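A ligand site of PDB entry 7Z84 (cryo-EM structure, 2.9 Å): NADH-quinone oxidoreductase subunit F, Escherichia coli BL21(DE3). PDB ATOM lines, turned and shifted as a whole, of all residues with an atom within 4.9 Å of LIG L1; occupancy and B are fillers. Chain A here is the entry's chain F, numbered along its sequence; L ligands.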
ATOM      1  N   GLY A  61      12.134   3.624  33.612  1.00  0.00           N
ATOM      2  CA  GLY A  61      13.126   4.058  32.658  1.00  0.00           C
ATOM      3  C   GLY A  61      12.498   4.817  31.508  1.00  0.00           C
ATOM      4  O   GLY A  61      11.551   4.332  30.858  1.00  0.00           O
ATOM      5  N   ARG A  62      13.005   6.015  31.238  1.00  0.00           N
ATOM      6  CA  ARG A  62      12.504   6.861  30.163  1.00  0.00           C
ATOM      7  C   ARG A  62      13.233   6.644  28.848  1.00  0.00           C
ATOM      8  O   ARG A  62      12.961   7.359  27.886  1.00  0.00           O
ATOM      9  CB  ARG A  62      12.599   8.326  30.563  1.00  0.00           C
ATOM     10  CG  ARG A  62      11.898   8.661  31.875  1.00  0.00           C
ATOM     11  CD  ARG A  62      10.413   8.438  31.767  1.00  0.00           C
ATOM     12  NE  ARG A  62       9.666   9.278  32.694  1.00  0.00           N
ATOM     13  CZ  ARG A  62       9.082   8.846  33.800  1.00  0.00           C
ATOM     14  NH1 ARG A  62       9.136   7.572  34.150  1.00  0.00           N
ATOM     15  NH2 ARG A  62       8.431   9.704  34.578  1.00  0.00           N
ATOM     16  N   GLY A  63      14.167   5.681  28.793  1.00  0.00           N
ATOM     17  CA  GLY A  63      14.842   5.389  27.538  1.00  0.00           C
ATOM     18  C   GLY A  63      13.926   4.796  26.489  1.00  0.00           C
ATOM     19  O   GLY A  63      14.118   5.026  25.290  1.00  0.00           O
ATOM     20  N   GLY A  64      12.921   4.040  26.917  1.00  0.00           N
ATOM     21  CA  GLY A  64      11.988   3.444  25.981  1.00  0.00           C
ATOM     22  C   GLY A  64      11.553   2.043  26.369  1.00  0.00           C
ATOM     23  O   GLY A  64      10.666   1.465  25.735  1.00  0.00           O
ATOM     24  N   ALA A  65      12.156   1.489  27.417  1.00  0.00           N
ATOM     25  CA  ALA A  65      11.837   0.138  27.855  1.00  0.00           C
ATOM     26  C   ALA A  65      10.957   0.100  29.095  1.00  0.00           C
ATOM     27  O   ALA A  65      10.252  -0.887  29.305  1.00  0.00           O
ATOM     28  CB  ALA A  65      13.114  -0.651  28.129  1.00  0.00           C
ATOM     29  N   PHE A  67      11.773  -0.064  32.301  1.00  0.00           N
ATOM     30  CA  PHE A  67      12.266  -0.756  33.481  1.00  0.00           C
ATOM     31  C   PHE A  67      12.371   0.215  34.648  1.00  0.00           C
ATOM     32  O   PHE A  67      12.748   1.379  34.480  1.00  0.00           O
ATOM     33  CB  PHE A  67      13.634  -1.388  33.187  1.00  0.00           C
ATOM     34  CG  PHE A  67      14.050  -2.430  34.181  1.00  0.00           C
ATOM     35  CD1 PHE A  67      13.418  -3.674  34.203  1.00  0.00           C
ATOM     36  CD2 PHE A  67      15.051  -2.176  35.099  1.00  0.00           C
ATOM     37  CE1 PHE A  67      13.793  -4.632  35.111  1.00  0.00           C
ATOM     38  CE2 PHE A  67      15.430  -3.145  36.016  1.00  0.00           C
ATOM     39  CZ  PHE A  67      14.804  -4.370  36.023  1.00  0.00           C
ATOM     40  N   THR A  69      13.707   2.172  37.723  1.00  0.00           N
ATOM     41  CA  THR A  69      15.054   2.649  38.009  1.00  0.00           C
ATOM     42  C   THR A  69      15.521   2.230  39.397  1.00  0.00           C
ATOM     43  O   THR A  69      16.717   1.956  39.592  1.00  0.00           O
ATOM     44  CB  THR A  69      15.107   4.167  37.858  1.00  0.00           C
ATOM     45  OG1 THR A  69      14.419   4.537  36.657  1.00  0.00           O
ATOM     46  CG2 THR A  69      16.543   4.653  37.763  1.00  0.00           C
ATOM     47  N   LYS A  72      16.769  -1.277  39.306  1.00  0.00           N
ATOM     48  CA  LYS A  72      18.059  -1.313  38.619  1.00  0.00           C
ATOM     49  C   LYS A  72      19.175  -0.810  39.534  1.00  0.00           C
ATOM     50  O   LYS A  72      20.304  -1.305  39.473  1.00  0.00           O
ATOM     51  CB  LYS A  72      18.006  -0.471  37.349  1.00  0.00           C
ATOM     52  CG  LYS A  72      19.152  -0.743  36.389  1.00  0.00           C
ATOM     53  CD  LYS A  72      19.440   0.457  35.520  1.00  0.00           C
ATOM     54  CE  LYS A  72      18.293   0.742  34.574  1.00  0.00           C
ATOM     55  NZ  LYS A  72      18.758   1.496  33.378  1.00  0.00           N
ATOM     56  N   ASN A  90      22.896   8.064  29.130  1.00  0.00           N
ATOM     57  CA  ASN A  90      22.713   7.718  27.730  1.00  0.00           C
ATOM     58  C   ASN A  90      22.117   8.923  27.005  1.00  0.00           C
ATOM     59  O   ASN A  90      20.922   8.983  26.709  1.00  0.00           O
ATOM     60  CB  ASN A  90      21.830   6.478  27.598  1.00  0.00           C
ATOM     61  CG  ASN A  90      21.999   5.763  26.284  1.00  0.00           C
ATOM     62  OD1 ASN A  90      22.339   6.380  25.271  1.00  0.00           O
ATOM     63  ND2 ASN A  90      21.780   4.458  26.290  1.00  0.00           N
ATOM     64  N   ASP A  92      22.724   9.658  24.006  1.00  0.00           N
ATOM     65  CA  ASP A  92      22.833   9.397  22.570  1.00  0.00           C
ATOM     66  C   ASP A  92      21.593   9.882  21.834  1.00  0.00           C
ATOM     67  O   ASP A  92      21.676  10.807  21.019  1.00  0.00           O
ATOM     68  CB  ASP A  92      23.059   7.897  22.327  1.00  0.00           C
ATOM     69  CG  ASP A  92      23.863   7.641  21.069  1.00  0.00           C
ATOM     70  OD1 ASP A  92      24.532   8.567  20.581  1.00  0.00           O
ATOM     71  OD2 ASP A  92      23.829   6.496  20.570  1.00  0.00           O
ATOM     72  N   GLU A  93      20.433   9.295  22.140  1.00  0.00           N
ATOM     73  CA  GLU A  93      19.134   9.689  21.577  1.00  0.00           C
ATOM     74  C   GLU A  93      19.153   9.669  20.049  1.00  0.00           C
ATOM     75  O   GLU A  93      18.843  10.660  19.388  1.00  0.00           O
ATOM     76  CB  GLU A  93      18.687  11.048  22.102  1.00  0.00           C
ATOM     77  CG  GLU A  93      17.182  11.222  22.151  1.00  0.00           C
ATOM     78  CD  GLU A  93      16.770  12.674  22.051  1.00  0.00           C
ATOM     79  OE1 GLU A  93      17.535  13.485  21.496  1.00  0.00           O
ATOM     80  OE2 GLU A  93      15.663  13.005  22.539  1.00  0.00           O
ATOM     81  N   MET A  94      19.533   8.531  19.499  1.00  0.00           N
ATOM     82  CA  MET A  94      19.706   8.394  18.063  1.00  0.00           C
ATOM     83  C   MET A  94      18.476   7.818  17.364  1.00  0.00           C
ATOM     84  O   MET A  94      18.525   7.600  16.148  1.00  0.00           O
ATOM     85  CB  MET A  94      20.933   7.516  17.765  1.00  0.00           C
ATOM     86  CG  MET A  94      22.211   8.290  17.547  1.00  0.00           C
ATOM     87  SD  MET A  94      22.557   8.546  15.797  1.00  0.00           S
ATOM     88  CE  MET A  94      24.288   8.974  15.866  1.00  0.00           C
ATOM     89  N   TYR A 178      24.278   4.737  15.631  1.00  0.00           N
ATOM     90  CA  TYR A 178      23.005   4.559  16.318  1.00  0.00           C
ATOM     91  C   TYR A 178      23.059   3.463  17.367  1.00  0.00           C
ATOM     92  O   TYR A 178      22.400   3.567  18.402  1.00  0.00           O
ATOM     93  CB  TYR A 178      21.905   4.270  15.294  1.00  0.00           C
ATOM     94  CG  TYR A 178      20.634   3.679  15.857  1.00  0.00           C
ATOM     95  CD1 TYR A 178      19.692   4.479  16.495  1.00  0.00           C
ATOM     96  CD2 TYR A 178      20.348   2.327  15.720  1.00  0.00           C
ATOM     97  CE1 TYR A 178      18.519   3.947  16.996  1.00  0.00           C
ATOM     98  CE2 TYR A 178      19.181   1.788  16.222  1.00  0.00           C
ATOM     99  CZ  TYR A 178      18.273   2.604  16.853  1.00  0.00           C
ATOM    100  OH  TYR A 178      17.109   2.067  17.345  1.00  0.00           O
ATOM    101  N   ILE A 179      23.840   2.403  17.117  1.00  0.00           N
ATOM    102  CA  ILE A 179      23.905   1.262  18.039  1.00  0.00           C
ATOM    103  C   ILE A 179      24.572   1.623  19.357  1.00  0.00           C
ATOM    104  O   ILE A 179      24.398   0.900  20.350  1.00  0.00           O
ATOM    105  CB  ILE A 179      24.615   0.096  17.335  1.00  0.00           C
ATOM    106  CG1 ILE A 179      24.354  -1.241  18.035  1.00  0.00           C
ATOM    107  CG2 ILE A 179      26.109   0.353  17.217  1.00  0.00           C
ATOM    108  CD1 ILE A 179      22.926  -1.451  18.479  1.00  0.00           C
ATOM    109  N   GLY A 181      23.657   3.727  21.446  1.00  0.00           N
ATOM    110  CA  GLY A 181      22.679   3.961  22.480  1.00  0.00           C
ATOM    111  C   GLY A 181      22.317   2.735  23.286  1.00  0.00           C
ATOM    112  O   GLY A 181      21.819   2.862  24.411  1.00  0.00           O
ATOM    113  N   GLU A 182      22.530   1.542  22.733  1.00  0.00           N
ATOM    114  CA  GLU A 182      22.400   0.308  23.502  1.00  0.00           C
ATOM    115  C   GLU A 182      23.420   0.312  24.629  1.00  0.00           C
ATOM    116  O   GLU A 182      24.592   0.590  24.404  1.00  0.00           O
ATOM    117  CB  GLU A 182      22.616  -0.911  22.596  1.00  0.00           C
ATOM    118  CG  GLU A 182      21.756  -2.101  22.940  1.00  0.00           C
ATOM    119  CD  GLU A 182      22.391  -3.016  23.963  1.00  0.00           C
ATOM    120  OE1 GLU A 182      23.584  -2.823  24.274  1.00  0.00           O
ATOM    121  OE2 GLU A 182      21.689  -3.917  24.469  1.00  0.00           O
ATOM    122  N   GLU A 183      22.948  -0.006  25.845  1.00  0.00           N
ATOM    123  CA  GLU A 183      23.723   0.290  27.049  1.00  0.00           C
ATOM    124  C   GLU A 183      25.024  -0.507  27.112  1.00  0.00           C
ATOM    125  O   GLU A 183      26.055   0.011  27.559  1.00  0.00           O
ATOM    126  CB  GLU A 183      22.873   0.050  28.297  1.00  0.00           C
ATOM    127  CG  GLU A 183      22.452  -1.393  28.494  1.00  0.00           C
ATOM    128  CD  GLU A 183      22.187  -1.726  29.934  1.00  0.00           C
ATOM    129  OE1 GLU A 183      21.377  -2.632  30.177  1.00  0.00           O
ATOM    130  OE2 GLU A 183      22.779  -1.074  30.821  1.00  0.00           O
ATOM    131  N   VAL A 216      23.577   2.559  33.872  1.00  0.00           N
ATOM    132  CA  VAL A 216      23.293   3.396  32.711  1.00  0.00           C
ATOM    133  C   VAL A 216      21.840   3.844  32.776  1.00  0.00           C
ATOM    134  O   VAL A 216      20.937   3.002  32.899  1.00  0.00           O
ATOM    135  CB  VAL A 216      23.586   2.657  31.397  1.00  0.00           C
ATOM    136  CG1 VAL A 216      23.421   3.587  30.213  1.00  0.00           C
ATOM    137  CG2 VAL A 216      24.980   2.050  31.433  1.00  0.00           C
ATOM    138  N   ASN A 217      21.605   5.147  32.702  1.00  0.00           N
ATOM    139  CA  ASN A 217      20.263   5.693  32.720  1.00  0.00           C
ATOM    140  C   ASN A 217      20.122   6.765  31.658  1.00  0.00           C
ATOM    141  O   ASN A 217      21.113   7.390  31.254  1.00  0.00           O
ATOM    142  CB  ASN A 217      19.900   6.276  34.099  1.00  0.00           C
ATOM    143  CG  ASN A 217      19.352   5.219  35.045  1.00  0.00           C
ATOM    144  OD1 ASN A 217      19.968   4.890  36.049  1.00  0.00           O
ATOM    145  ND2 ASN A 217      18.180   4.697  34.726  1.00  0.00           N
ATOM    146  N   ASN A 218      18.890   6.979  31.208  1.00  0.00           N
ATOM    147  CA  ASN A 218      18.601   7.999  30.204  1.00  0.00           C
ATOM    148  C   ASN A 218      18.693   9.396  30.823  1.00  0.00           C
ATOM    149  O   ASN A 218      18.754   9.566  32.049  1.00  0.00           O
ATOM    150  CB  ASN A 218      17.224   7.761  29.594  1.00  0.00           C
ATOM    151  CG  ASN A 218      17.035   8.481  28.268  1.00  0.00           C
ATOM    152  OD1 ASN A 218      17.996   8.957  27.663  1.00  0.00           O
ATOM    153  ND2 ASN A 218      15.797   8.582  27.828  1.00  0.00           N
ATOM    154  N   THR A 221      15.290  10.197  32.839  1.00  0.00           N
ATOM    155  CA  THR A 221      15.195   9.573  34.156  1.00  0.00           C
ATOM    156  C   THR A 221      16.014  10.334  35.188  1.00  0.00           C
ATOM    157  O   THR A 221      15.543  10.619  36.299  1.00  0.00           O
ATOM    158  CB  THR A 221      15.668   8.120  34.069  1.00  0.00           C
ATOM    159  OG1 THR A 221      14.988   7.455  32.999  1.00  0.00           O
ATOM    160  CG2 THR A 221      15.378   7.389  35.359  1.00  0.00           C
ATOM    161  N   CYS A 398      20.827  -8.605  20.154  1.00  0.00           N
ATOM    162  CA  CYS A 398      20.320  -7.472  20.912  1.00  0.00           C
ATOM    163  C   CYS A 398      18.932  -7.130  20.383  1.00  0.00           C
ATOM    164  O   CYS A 398      18.376  -7.831  19.537  1.00  0.00           O
ATOM    165  CB  CYS A 398      21.307  -6.301  20.841  1.00  0.00           C
ATOM    166  SG  CYS A 398      21.055  -5.142  19.497  1.00  0.00           S
ATOM    167  N   ALA A 399      18.356  -6.033  20.881  1.00  0.00           N
ATOM    168  CA  ALA A 399      16.983  -5.664  20.592  1.00  0.00           C
ATOM    169  C   ALA A 399      16.857  -4.659  19.451  1.00  0.00           C
ATOM    170  O   ALA A 399      15.809  -4.027  19.304  1.00  0.00           O
ATOM    171  CB  ALA A 399      16.299  -5.113  21.839  1.00  0.00           C
ATOM    172  N   HIS A 400      17.912  -4.489  18.649  1.00  0.00           N
ATOM    173  CA  HIS A 400      17.847  -3.564  17.528  1.00  0.00           C
ATOM    174  C   HIS A 400      16.958  -4.094  16.407  1.00  0.00           C
ATOM    175  O   HIS A 400      16.144  -3.349  15.845  1.00  0.00           O
ATOM    176  CB  HIS A 400      19.263  -3.299  17.019  1.00  0.00           C
ATOM    177  CG  HIS A 400      19.318  -2.696  15.651  1.00  0.00           C
ATOM    178  ND1 HIS A 400      19.519  -3.448  14.522  1.00  0.00           N
ATOM    179  CD2 HIS A 400      19.231  -1.412  15.239  1.00  0.00           C
ATOM    180  CE1 HIS A 400      19.534  -2.653  13.465  1.00  0.00           C
ATOM    181  NE2 HIS A 400      19.361  -1.412  13.871  1.00  0.00           N
HETATM  182  N1  LIG L   1      18.512   4.464  25.398  1.00  0.00           N
HETATM  183  C1  LIG L   1      18.793   5.811  25.424  1.00  0.00           C
HETATM  184  O1  LIG L   1      18.596   6.445  26.447  1.00  0.00           O
HETATM  185  N2  LIG L   1      19.290   6.433  24.299  1.00  0.00           N
HETATM  186  C2  LIG L   1      19.507   5.695  23.146  1.00  0.00           C
HETATM  187  O2  LIG L   1      19.947   6.253  22.148  1.00  0.00           O
HETATM  188  C3  LIG L   1      19.223   4.346  23.130  1.00  0.00           C
HETATM  189  N3  LIG L   1      19.431   3.613  21.985  1.00  0.00           N
HETATM  190  C4  LIG L   1      19.154   2.256  21.969  1.00  0.00           C
HETATM  191  C5  LIG L   1      19.374   1.547  20.814  1.00  0.00           C
HETATM  192  C6  LIG L   1      19.099   0.192  20.767  1.00  0.00           C
HETATM  193  C7  LIG L   1      19.344  -0.575  19.506  1.00  0.00           C
HETATM  194  C8  LIG L   1      18.598  -0.446  21.897  1.00  0.00           C
HETATM  195  C9  LIG L   1      18.286  -1.915  21.861  1.00  0.00           C
HETATM  196  C10 LIG L   1      18.375   0.273  23.065  1.00  0.00           C
HETATM  197  C11 LIG L   1      18.653   1.631  23.103  1.00  0.00           C
HETATM  198  N4  LIG L   1      18.436   2.369  24.257  1.00  0.00           N
HETATM  199  C12 LIG L   1      18.723   3.721  24.263  1.00  0.00           C
HETATM  200  C13 LIG L   1      17.901   1.741  25.509  1.00  0.00           C
HETATM  201  C14 LIG L   1      19.053   1.312  26.416  1.00  0.00           C
HETATM  202  O3  LIG L   1      19.396  -0.031  26.156  1.00  0.00           O
HETATM  203  C15 LIG L   1      18.706   1.468  27.900  1.00  0.00           C
HETATM  204  O4  LIG L   1      17.379   1.052  28.103  1.00  0.00           O
HETATM  205  C16 LIG L   1      18.872   2.916  28.329  1.00  0.00           C
HETATM  206  O5  LIG L   1      20.082   3.427  27.822  1.00  0.00           O
HETATM  207  C17 LIG L   1      18.853   3.110  29.840  1.00  0.00           C
HETATM  208  O6  LIG L   1      17.665   2.579  30.392  1.00  0.00           O
HETATM  209  P1  LIG L   1      16.659   3.536  31.182  1.00  0.00           P
HETATM  210  O7  LIG L   1      15.438   3.730  30.329  1.00  0.00           O
HETATM  211  O8  LIG L   1      16.274   2.922  32.507  1.00  0.00           O
HETATM  212  O9  LIG L   1      17.296   4.881  31.428  1.00  0.00           O
HETATM  213  P1  LG2 L   2      15.673  -4.170  28.156  1.00  0.00           P
HETATM  214  O1  LG2 L   2      14.249  -3.817  28.268  1.00  0.00           O
HETATM  215  O2  LG2 L   2      16.008  -5.624  28.448  1.00  0.00           O
HETATM  216  O3  LG2 L   2      16.578  -3.292  29.161  1.00  0.00           O
HETATM  217  C1  LG2 L   2      16.172  -1.991  29.628  1.00  0.00           C
HETATM  218  C2  LG2 L   2      16.803  -1.742  30.980  1.00  0.00           C
HETATM  219  O4  LG2 L   2      16.329  -2.733  31.924  1.00  0.00           O
HETATM  220  C3  LG2 L   2      18.329  -1.791  31.006  1.00  0.00           C
HETATM  221  O5  LG2 L   2      18.877  -0.683  31.711  1.00  0.00           O
HETATM  222  C4  LG2 L   2      18.626  -3.128  31.697  1.00  0.00           C
HETATM  223  O6  LG2 L   2      19.835  -3.078  32.440  1.00  0.00           O
HETATM  224  C5  LG2 L   2      17.424  -3.267  32.634  1.00  0.00           C
HETATM  225  N1  LG2 L   2      17.118  -4.647  32.992  1.00  0.00           N
HETATM  226  C6  LG2 L   2      16.161  -5.448  32.448  1.00  0.00           C
HETATM  227  N2  LG2 L   2      16.097  -6.652  32.975  1.00  0.00           N
HETATM  228  C7  LG2 L   2      17.090  -6.633  33.945  1.00  0.00           C
HETATM  229  C8  LG2 L   2      17.543  -7.589  34.867  1.00  0.00           C
HETATM  230  N3  LG2 L   2      17.029  -8.822  34.972  1.00  0.00           N
HETATM  231  N4  LG2 L   2      18.560  -7.255  35.681  1.00  0.00           N
HETATM  232  C9  LG2 L   2      19.088  -6.024  35.580  1.00  0.00           C
HETATM  233  N5  LG2 L   2      18.740  -5.040  34.764  1.00  0.00           N
HETATM  234  C10 LG2 L   2      17.737  -5.402  33.968  1.00  0.00           C
HETATM  235  O7  LG2 L   2      16.231  -3.858  26.694  1.00  0.00           O
HETATM  236  P2  LG2 L   2      17.197  -2.763  26.054  1.00  0.00           P
HETATM  237  O8  LG2 L   2      17.776  -3.380  24.788  1.00  0.00           O
HETATM  238  O9  LG2 L   2      18.211  -2.283  27.005  1.00  0.00           O
HETATM  239  O10 LG2 L   2      16.225  -1.582  25.572  1.00  0.00           O
HETATM  240  C11 LG2 L   2      15.149  -1.795  24.642  1.00  0.00           C
HETATM  241  C12 LG2 L   2      14.348  -0.528  24.520  1.00  0.00           C
HETATM  242  O11 LG2 L   2      15.162   0.513  23.979  1.00  0.00           O
HETATM  243  C13 LG2 L   2      13.133  -0.611  23.581  1.00  0.00           C
HETATM  244  O12 LG2 L   2      11.947  -0.911  24.306  1.00  0.00           O
HETATM  245  C14 LG2 L   2      13.072   0.790  22.939  1.00  0.00           C
HETATM  246  O13 LG2 L   2      11.874   1.480  23.302  1.00  0.00           O
HETATM  247  C15 LG2 L   2      14.299   1.509  23.492  1.00  0.00           C
HETATM  248  N6  LG2 L   2      15.016   2.287  22.480  1.00  0.00           N
HETATM  249  C16 LG2 L   2      15.336   3.630  22.701  1.00  0.00           C
HETATM  250  C17 LG2 L   2      15.988   4.392  21.804  1.00  0.00           C
HETATM  251  C18 LG2 L   2      16.252   5.805  22.168  1.00  0.00           C
HETATM  252  O14 LG2 L   2      15.758   6.283  23.194  1.00  0.00           O
HETATM  253  N7  LG2 L   2      17.015   6.518  21.358  1.00  0.00           N
HETATM  254  C19 LG2 L   2      16.422   3.819  20.494  1.00  0.00           C
HETATM  255  C20 LG2 L   2      16.022   2.391  20.343  1.00  0.00           C
HETATM  256  C21 LG2 L   2      15.372   1.726  21.289  1.00  0.00           C
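The backbone NH (N) of Gly 61 lies within hydrogen-bond range of the backbone carbonyl oxygen (O) of Phe 67, 2.5 Å away. The side-chain amide oxygen (OD1) of Asn 218 lies close to the backbone carbonyl oxygen (O) of Asn 90, 3.1 Å away. The backbone NH of Gly 181 is in hydrogen-bond range of the side-chain carboxylate of Asp 92, at 2.9 Å. The backbone NH of His 400 lies close to the side-chain sulfur of Cys 398, at 3.3 Å. The side-chain amino group (NZ) of Lys 72 lies within hydrogen-bond range of the backbone carbonyl oxygen (O) of Val 216, at 2.7 Å. The side-chain amide nitrogen of Asn 218 lies within hydrogen-bond range of the backbone carbonyl oxygen of Arg 62, at 3.1 Å. The backbone NH of Asn 90 sits at hydrogen-bond distance from the backbone carbonyl oxygen of Asn 217, 2.9 Å away. The backbone NH of Arg 62 sits at hydrogen-bond distance from the side-chain hydroxyl of Thr 221 (3.0 Å).
N of Glu 93 lies within hydrogen-bond range of O2 of LIG L1 (3.1 Å). O5 of LIG L1 lies within hydrogen-bond range of ND2 of Asn 90, at 2.5 Å. The side-chain amide oxygen (OD1) of Asn 218 lies close to an oxygen (O1) of LIG L1, at 2.9 Å. The side-chain carboxylate of Glu 183 is in hydrogen-bond range of an oxygen (O6) of LG2 L2. N of Asn 218 sits at hydrogen-bond distance from O9 of LIG L1 (2.6 Å). An oxygen (O13) of LG2 L2 is in hydrogen-bond range of the backbone carbonyl oxygen (O) of Gly 64 (2.7 Å). The backbone NH (N) of Gly 63 is in hydrogen-bond range of an oxygen (O7) of LIG L1, 2.8 Å away. The side-chain amino group (NZ) of Lys 72 is in salt-bridge range of an oxygen (O8) of LIG L1 (3.0 Å). The side-chain amino group (NZ) of Lys 72 sits at hydrogen-bond distance from an oxygen (O5) of LG2 L2. The side-chain amide nitrogen (ND2) of Asn 217 lies close to an oxygen (O9) of LIG L1, 3.4 Å away. N of Arg 62 lies within hydrogen-bond range of O7 of LIG L1, at 3.5 Å.
An oxygen (O3) of LIG L1 lies within hydrogen-bond range of an oxygen (O9) of LG2 L2 (2.7 Å).
O of Gly 181 sits close to N4 of LIG L1, 3.4 Å away. Merely in contact with LIG L1: Gly 61 (3.3 Å), Asp 92 (3.5 Å), Met 94 (3.5 Å), Ile 179 (3.8 Å), Glu 182 (3.5 Å), Glu 183 (3.6 Å), Val 216 (3.7 Å), Thr 221 (3.8 Å), Ala 399 (3.8 Å) and His 400 (3.7 Å). Hydrophobic or aromatic side chains that line LIG L1: Ile 179, Ala 399 and His 400. Of the 24 residues printed, 18 come within 4 Å of LIG L1. Along chain A the residues within 4 Å of LIG L1 span positions 61 to 400.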
